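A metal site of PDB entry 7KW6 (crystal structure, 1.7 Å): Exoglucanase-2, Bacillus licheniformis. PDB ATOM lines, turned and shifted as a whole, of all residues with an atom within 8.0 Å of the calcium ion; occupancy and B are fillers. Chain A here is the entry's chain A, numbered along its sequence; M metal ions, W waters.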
ATOM      1  N   PRO A 113       9.914   1.916  -4.028  1.00  0.00           N
ATOM      2  CA  PRO A 113      10.895   0.891  -3.631  1.00  0.00           C
ATOM      3  C   PRO A 113      11.696   0.316  -4.780  1.00  0.00           C
ATOM      4  O   PRO A 113      12.658  -0.421  -4.509  1.00  0.00           O
ATOM      5  CB  PRO A 113      10.031  -0.195  -2.957  1.00  0.00           C
ATOM      6  CG  PRO A 113       8.613  -0.009  -3.556  1.00  0.00           C
ATOM      7  CD  PRO A 113       8.507   1.484  -3.803  1.00  0.00           C
ATOM      8  N   TYR A 114      11.379   0.634  -6.045  1.00  0.00           N
ATOM      9  CA  TYR A 114      12.190   0.225  -7.191  1.00  0.00           C
ATOM     10  C   TYR A 114      12.267   1.373  -8.174  1.00  0.00           C
ATOM     11  O   TYR A 114      11.318   2.140  -8.313  1.00  0.00           O
ATOM     12  CB  TYR A 114      11.608  -0.988  -7.946  1.00  0.00           C
ATOM     13  CG  TYR A 114      11.429  -2.182  -7.067  1.00  0.00           C
ATOM     14  CD1 TYR A 114      12.528  -2.960  -6.701  1.00  0.00           C
ATOM     15  CD2 TYR A 114      10.167  -2.514  -6.550  1.00  0.00           C
ATOM     16  CE1 TYR A 114      12.381  -4.049  -5.853  1.00  0.00           C
ATOM     17  CE2 TYR A 114      10.032  -3.598  -5.698  1.00  0.00           C
ATOM     18  CZ  TYR A 114      11.138  -4.352  -5.366  1.00  0.00           C
ATOM     19  OH  TYR A 114      10.983  -5.431  -4.536  1.00  0.00           O
ATOM     20  N   PRO A 115      13.355   1.473  -8.918  1.00  0.00           N
ATOM     21  CA  PRO A 115      13.429   2.517  -9.975  1.00  0.00           C
ATOM     22  C   PRO A 115      12.379   2.384 -11.035  1.00  0.00           C
ATOM     23  O   PRO A 115      11.989   3.379 -11.679  1.00  0.00           O
ATOM     24  CB  PRO A 115      14.830   2.333 -10.587  1.00  0.00           C
ATOM     25  CG  PRO A 115      15.598   1.503  -9.582  1.00  0.00           C
ATOM     26  CD  PRO A 115      14.582   0.660  -8.804  1.00  0.00           C
ATOM     27  N   ASP A 116      11.969   1.108 -11.377  1.00  0.00           N
ATOM     28  CA  ASP A 116      10.798   0.693 -12.139  1.00  0.00           C
ATOM     29  C   ASP A 116       9.568   1.573 -12.011  1.00  0.00           C
ATOM     30  O   ASP A 116       8.798   1.684 -12.925  1.00  0.00           O
ATOM     31  CB  ASP A 116      10.514  -0.759 -11.718  1.00  0.00           C
ATOM     32  CG  ASP A 116      11.426  -1.812 -12.236  1.00  0.00           C
ATOM     33  OD1 ASP A 116      12.111  -2.138 -13.189  1.00  0.00           O
ATOM     34  OD2 ASP A 116      12.475  -1.551 -11.472  1.00  0.00           O
ATOM     35  N   GLY A 180      15.078   6.361  -5.790  1.00  0.00           N
ATOM     36  CA  GLY A 180      14.738   5.624  -4.581  1.00  0.00           C
ATOM     37  C   GLY A 180      15.767   4.612  -4.121  1.00  0.00           C
ATOM     38  O   GLY A 180      16.880   4.502  -4.655  1.00  0.00           O
ATOM     39  N   GLU A 181      15.348   3.812  -3.129  1.00  0.00           N
ATOM     40  CA  GLU A 181      16.282   3.061  -2.303  1.00  0.00           C
ATOM     41  C   GLU A 181      16.926   1.913  -3.058  1.00  0.00           C
ATOM     42  O   GLU A 181      17.946   1.411  -2.611  1.00  0.00           O
ATOM     43  CB  GLU A 181      15.560   2.507  -1.047  1.00  0.00           C
ATOM     44  CG  GLU A 181      14.500   1.431  -1.360  1.00  0.00           C
ATOM     45  CD  GLU A 181      13.497   1.296  -0.232  1.00  0.00           C
ATOM     46  OE1 GLU A 181      13.588   2.091   0.732  1.00  0.00           O
ATOM     47  OE2 GLU A 181      12.620   0.412  -0.310  1.00  0.00           O
ATOM     48  N   GLN A 182      16.333   1.470  -4.166  1.00  0.00           N
ATOM     49  CA  GLN A 182      16.930   0.332  -4.856  1.00  0.00           C
ATOM     50  C   GLN A 182      17.751   0.765  -6.065  1.00  0.00           C
ATOM     51  O   GLN A 182      18.267  -0.095  -6.781  1.00  0.00           O
ATOM     52  CB  GLN A 182      15.812  -0.651  -5.288  1.00  0.00           C
ATOM     53  CG  GLN A 182      15.582  -1.725  -4.225  1.00  0.00           C
ATOM     54  CD  GLN A 182      16.852  -2.630  -4.143  1.00  0.00           C
ATOM     55  OE1 GLN A 182      17.559  -2.784  -5.143  1.00  0.00           O
ATOM     56  NE2 GLN A 182      17.107  -3.202  -3.007  1.00  0.00           N
ATOM     57  N   GLU A 183      17.900   2.067  -6.298  1.00  0.00           N
ATOM     58  CA  GLU A 183      18.670   2.530  -7.457  1.00  0.00           C
ATOM     59  C   GLU A 183      20.141   2.602  -7.053  1.00  0.00           C
ATOM     60  O   GLU A 183      20.635   3.629  -6.564  1.00  0.00           O
ATOM     61  CB  GLU A 183      18.157   3.883  -7.917  1.00  0.00           C
ATOM     62  CG  GLU A 183      18.732   4.282  -9.281  1.00  0.00           C
ATOM     63  CD  GLU A 183      18.376   5.723  -9.615  1.00  0.00           C
ATOM     64  OE1 GLU A 183      18.427   6.637  -8.738  1.00  0.00           O
ATOM     65  OE2 GLU A 183      18.115   5.945 -10.805  1.00  0.00           O
ATOM     66  N   SER A 184      20.871   1.505  -7.249  1.00  0.00           N
ATOM     67  CA  SER A 184      22.306   1.507  -6.995  1.00  0.00           C
ATOM     68  C   SER A 184      23.025   2.428  -7.965  1.00  0.00           C
ATOM     69  O   SER A 184      22.455   2.913  -8.927  1.00  0.00           O
ATOM     70  CB  SER A 184      22.891   0.110  -7.152  1.00  0.00           C
ATOM     71  OG  SER A 184      22.904  -0.280  -8.528  1.00  0.00           O
ATOM     72  N   VAL A 185      24.339   2.586  -7.746  1.00  0.00           N
ATOM     73  CA  VAL A 185      25.195   3.333  -8.654  1.00  0.00           C
ATOM     74  C   VAL A 185      25.063   2.819 -10.082  1.00  0.00           C
ATOM     75  O   VAL A 185      25.205   3.601 -11.032  1.00  0.00           O
ATOM     76  CB  VAL A 185      26.662   3.282  -8.169  1.00  0.00           C
ATOM     77  CG1 VAL A 185      27.228   1.845  -8.192  1.00  0.00           C
ATOM     78  CG2 VAL A 185      27.557   4.278  -8.974  1.00  0.00           C
ATOM     79  N   TRP A 186      24.785   1.512 -10.241  1.00  0.00           N
ATOM     80  CA  TRP A 186      24.691   0.874 -11.541  1.00  0.00           C
ATOM     81  C   TRP A 186      23.418   1.202 -12.287  1.00  0.00           C
ATOM     82  O   TRP A 186      23.296   0.831 -13.473  1.00  0.00           O
ATOM     83  CB  TRP A 186      24.740  -0.662 -11.361  1.00  0.00           C
ATOM     84  CG  TRP A 186      25.971  -1.066 -10.510  1.00  0.00           C
ATOM     85  CD1 TRP A 186      26.003  -1.398  -9.180  1.00  0.00           C
ATOM     86  CD2 TRP A 186      27.307  -1.139 -10.986  1.00  0.00           C
ATOM     87  NE1 TRP A 186      27.325  -1.666  -8.796  1.00  0.00           N
ATOM     88  CE2 TRP A 186      28.135  -1.483  -9.890  1.00  0.00           C
ATOM     89  CE3 TRP A 186      27.894  -0.947 -12.249  1.00  0.00           C
ATOM     90  CZ2 TRP A 186      29.498  -1.703 -10.044  1.00  0.00           C
ATOM     91  CZ3 TRP A 186      29.254  -1.141 -12.383  1.00  0.00           C
ATOM     92  CH2 TRP A 186      30.039  -1.491 -11.292  1.00  0.00           C
ATOM     93  N   GLU A 187      22.435   1.777 -11.609  1.00  0.00           N
ATOM     94  CA  GLU A 187      21.063   1.767 -12.131  1.00  0.00           C
ATOM     95  C   GLU A 187      20.553   3.152 -12.480  1.00  0.00           C
ATOM     96  O   GLU A 187      19.376   3.310 -12.797  1.00  0.00           O
ATOM     97  CB  GLU A 187      20.139   1.123 -11.091  1.00  0.00           C
ATOM     98  CG  GLU A 187      20.227  -0.408 -11.034  1.00  0.00           C
ATOM     99  CD  GLU A 187      19.591  -0.962  -9.737  1.00  0.00           C
ATOM    100  OE1 GLU A 187      18.368  -1.186  -9.714  1.00  0.00           O
ATOM    101  OE2 GLU A 187      20.325  -1.159  -8.753  1.00  0.00           O
ATOM    102  N   HIS A 405      19.337   0.658  -0.198  1.00  0.00           N
ATOM    103  CA  HIS A 405      19.323  -0.759   0.121  1.00  0.00           C
ATOM    104  C   HIS A 405      20.168  -1.580  -0.830  1.00  0.00           C
ATOM    105  O   HIS A 405      20.227  -2.813  -0.678  1.00  0.00           O
ATOM    106  CB  HIS A 405      17.885  -1.298   0.117  1.00  0.00           C
ATOM    107  CG  HIS A 405      17.006  -0.661   1.153  1.00  0.00           C
ATOM    108  ND1 HIS A 405      15.655  -0.966   1.251  1.00  0.00           N
ATOM    109  CD2 HIS A 405      17.266   0.238   2.142  1.00  0.00           C
ATOM    110  CE1 HIS A 405      15.118  -0.270   2.235  1.00  0.00           C
ATOM    111  NE2 HIS A 405      16.063   0.484   2.776  1.00  0.00           N
ATOM    112  N   ASP A 406      20.798  -0.943  -1.813  1.00  0.00           N
ATOM    113  CA  ASP A 406      21.532  -1.677  -2.859  1.00  0.00           C
ATOM    114  C   ASP A 406      22.891  -1.031  -3.068  1.00  0.00           C
ATOM    115  O   ASP A 406      23.080  -0.234  -4.008  1.00  0.00           O
ATOM    116  CB  ASP A 406      20.689  -1.695  -4.134  1.00  0.00           C
ATOM    117  CG  ASP A 406      21.250  -2.611  -5.204  1.00  0.00           C
ATOM    118  OD1 ASP A 406      22.221  -3.352  -4.932  1.00  0.00           O
ATOM    119  OD2 ASP A 406      20.666  -2.589  -6.319  1.00  0.00           O
ATOM    120  N   PRO A 407      23.890  -1.374  -2.236  1.00  0.00           N
ATOM    121  CA  PRO A 407      23.831  -2.248  -1.055  1.00  0.00           C
ATOM    122  C   PRO A 407      23.316  -1.468   0.137  1.00  0.00           C
ATOM    123  O   PRO A 407      23.276  -0.254   0.121  1.00  0.00           O
ATOM    124  CB  PRO A 407      25.318  -2.642  -0.846  1.00  0.00           C
ATOM    125  CG  PRO A 407      26.035  -1.445  -1.295  1.00  0.00           C
ATOM    126  CD  PRO A 407      25.233  -0.815  -2.416  1.00  0.00           C
ATOM    127  N   ARG A 598      28.253  -6.069 -12.476  1.00  0.00           N
ATOM    128  CA  ARG A 598      27.182  -5.138 -12.799  1.00  0.00           C
ATOM    129  C   ARG A 598      27.567  -4.136 -13.888  1.00  0.00           C
ATOM    130  O   ARG A 598      26.733  -3.281 -14.240  1.00  0.00           O
ATOM    131  CB  ARG A 598      26.688  -4.432 -11.527  1.00  0.00           C
ATOM    132  CG  ARG A 598      26.210  -5.491 -10.524  1.00  0.00           C
ATOM    133  CD  ARG A 598      25.652  -4.890  -9.223  1.00  0.00           C
ATOM    134  NE  ARG A 598      24.313  -4.358  -9.418  1.00  0.00           N
ATOM    135  CZ  ARG A 598      23.584  -3.910  -8.399  1.00  0.00           C
ATOM    136  NH1 ARG A 598      24.087  -3.968  -7.165  1.00  0.00           N
ATOM    137  NH2 ARG A 598      22.342  -3.470  -8.610  1.00  0.00           N
ATOM    138  N   GLU A 603      20.036  -3.783 -16.204  1.00  0.00           N
ATOM    139  CA  GLU A 603      19.265  -3.381 -15.046  1.00  0.00           C
ATOM    140  C   GLU A 603      19.071  -1.865 -14.988  1.00  0.00           C
ATOM    141  O   GLU A 603      18.610  -1.363 -13.956  1.00  0.00           O
ATOM    142  CB  GLU A 603      19.921  -3.891 -13.750  1.00  0.00           C
ATOM    143  CG  GLU A 603      21.344  -3.323 -13.509  1.00  0.00           C
ATOM    144  CD  GLU A 603      21.880  -3.790 -12.143  1.00  0.00           C
ATOM    145  OE1 GLU A 603      21.204  -3.537 -11.133  1.00  0.00           O
ATOM    146  OE2 GLU A 603      22.964  -4.418 -12.086  1.00  0.00           O
ATOM    147  N   LYS A 632       8.418  -5.828 -10.177  1.00  0.00           N
ATOM    148  CA  LYS A 632       8.867  -4.548  -9.635  1.00  0.00           C
ATOM    149  C   LYS A 632       7.936  -3.401 -10.010  1.00  0.00           C
ATOM    150  O   LYS A 632       8.256  -2.239  -9.732  1.00  0.00           O
ATOM    151  CB  LYS A 632      10.296  -4.259 -10.099  1.00  0.00           C
ATOM    152  CG  LYS A 632      11.327  -5.237  -9.560  1.00  0.00           C
ATOM    153  CD  LYS A 632      12.706  -4.997 -10.134  1.00  0.00           C
ATOM    154  CE  LYS A 632      13.768  -5.667  -9.330  1.00  0.00           C
ATOM    155  NZ  LYS A 632      13.876  -7.060  -9.713  1.00  0.00           N
HETATM  156 CA    CA M   1      18.596  -2.392  -7.451  1.00  0.00          CA
HETATM  157  O   HOH W   1      18.325  -4.686  -6.879  1.00  0.00           O
HETATM  158  O   HOH W   2      16.173  -2.650  -8.235  1.00  0.00           O
HETATM  159  O   HOH W   3      19.301  -4.070  -9.319  1.00  0.00           O
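OG of Ser 184 sits close to OE2 of Glu 187, at 2.7 Å. The side-chain carboxylate (OD1) of Asp 406 is in salt-bridge range of the guanidinium group (NH1) of Arg 598, at 3.0 Å. OE2 of Glu 187 sits close to NH2 of Arg 598 (3.1 Å).
Three residues have an atom within 4 Å of the calcium ion: Gln 182, Glu 187 and Asp 406. The nearest printed residue that does not touch the calcium ion is Arg 598 (4.1 Å).
The calcium ion is bound by the side-chain carboxylate (OD2) of Asp 406 (2.4 Å), water W1 (2.4 Å), the backbone carbonyl oxygen (O) of Gln 182 (2.4 Å), the side-chain carboxylate (OE2) of Glu 187 (2.5 Å), water W2 (2.6 Å), the side-chain amide oxygen (OE1) of Gln 182 (2.6 Å), the side-chain carboxylate (OE1) of Glu 187 (2.6 Å) and water W3 (2.6 Å). The calcium ion has eight donor atoms within binding distance.
Water W3 lies within hydrogen-bond range of OE1 of Glu 603 (2.7 Å) and NH2 of Arg 598 (3.2 Å).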
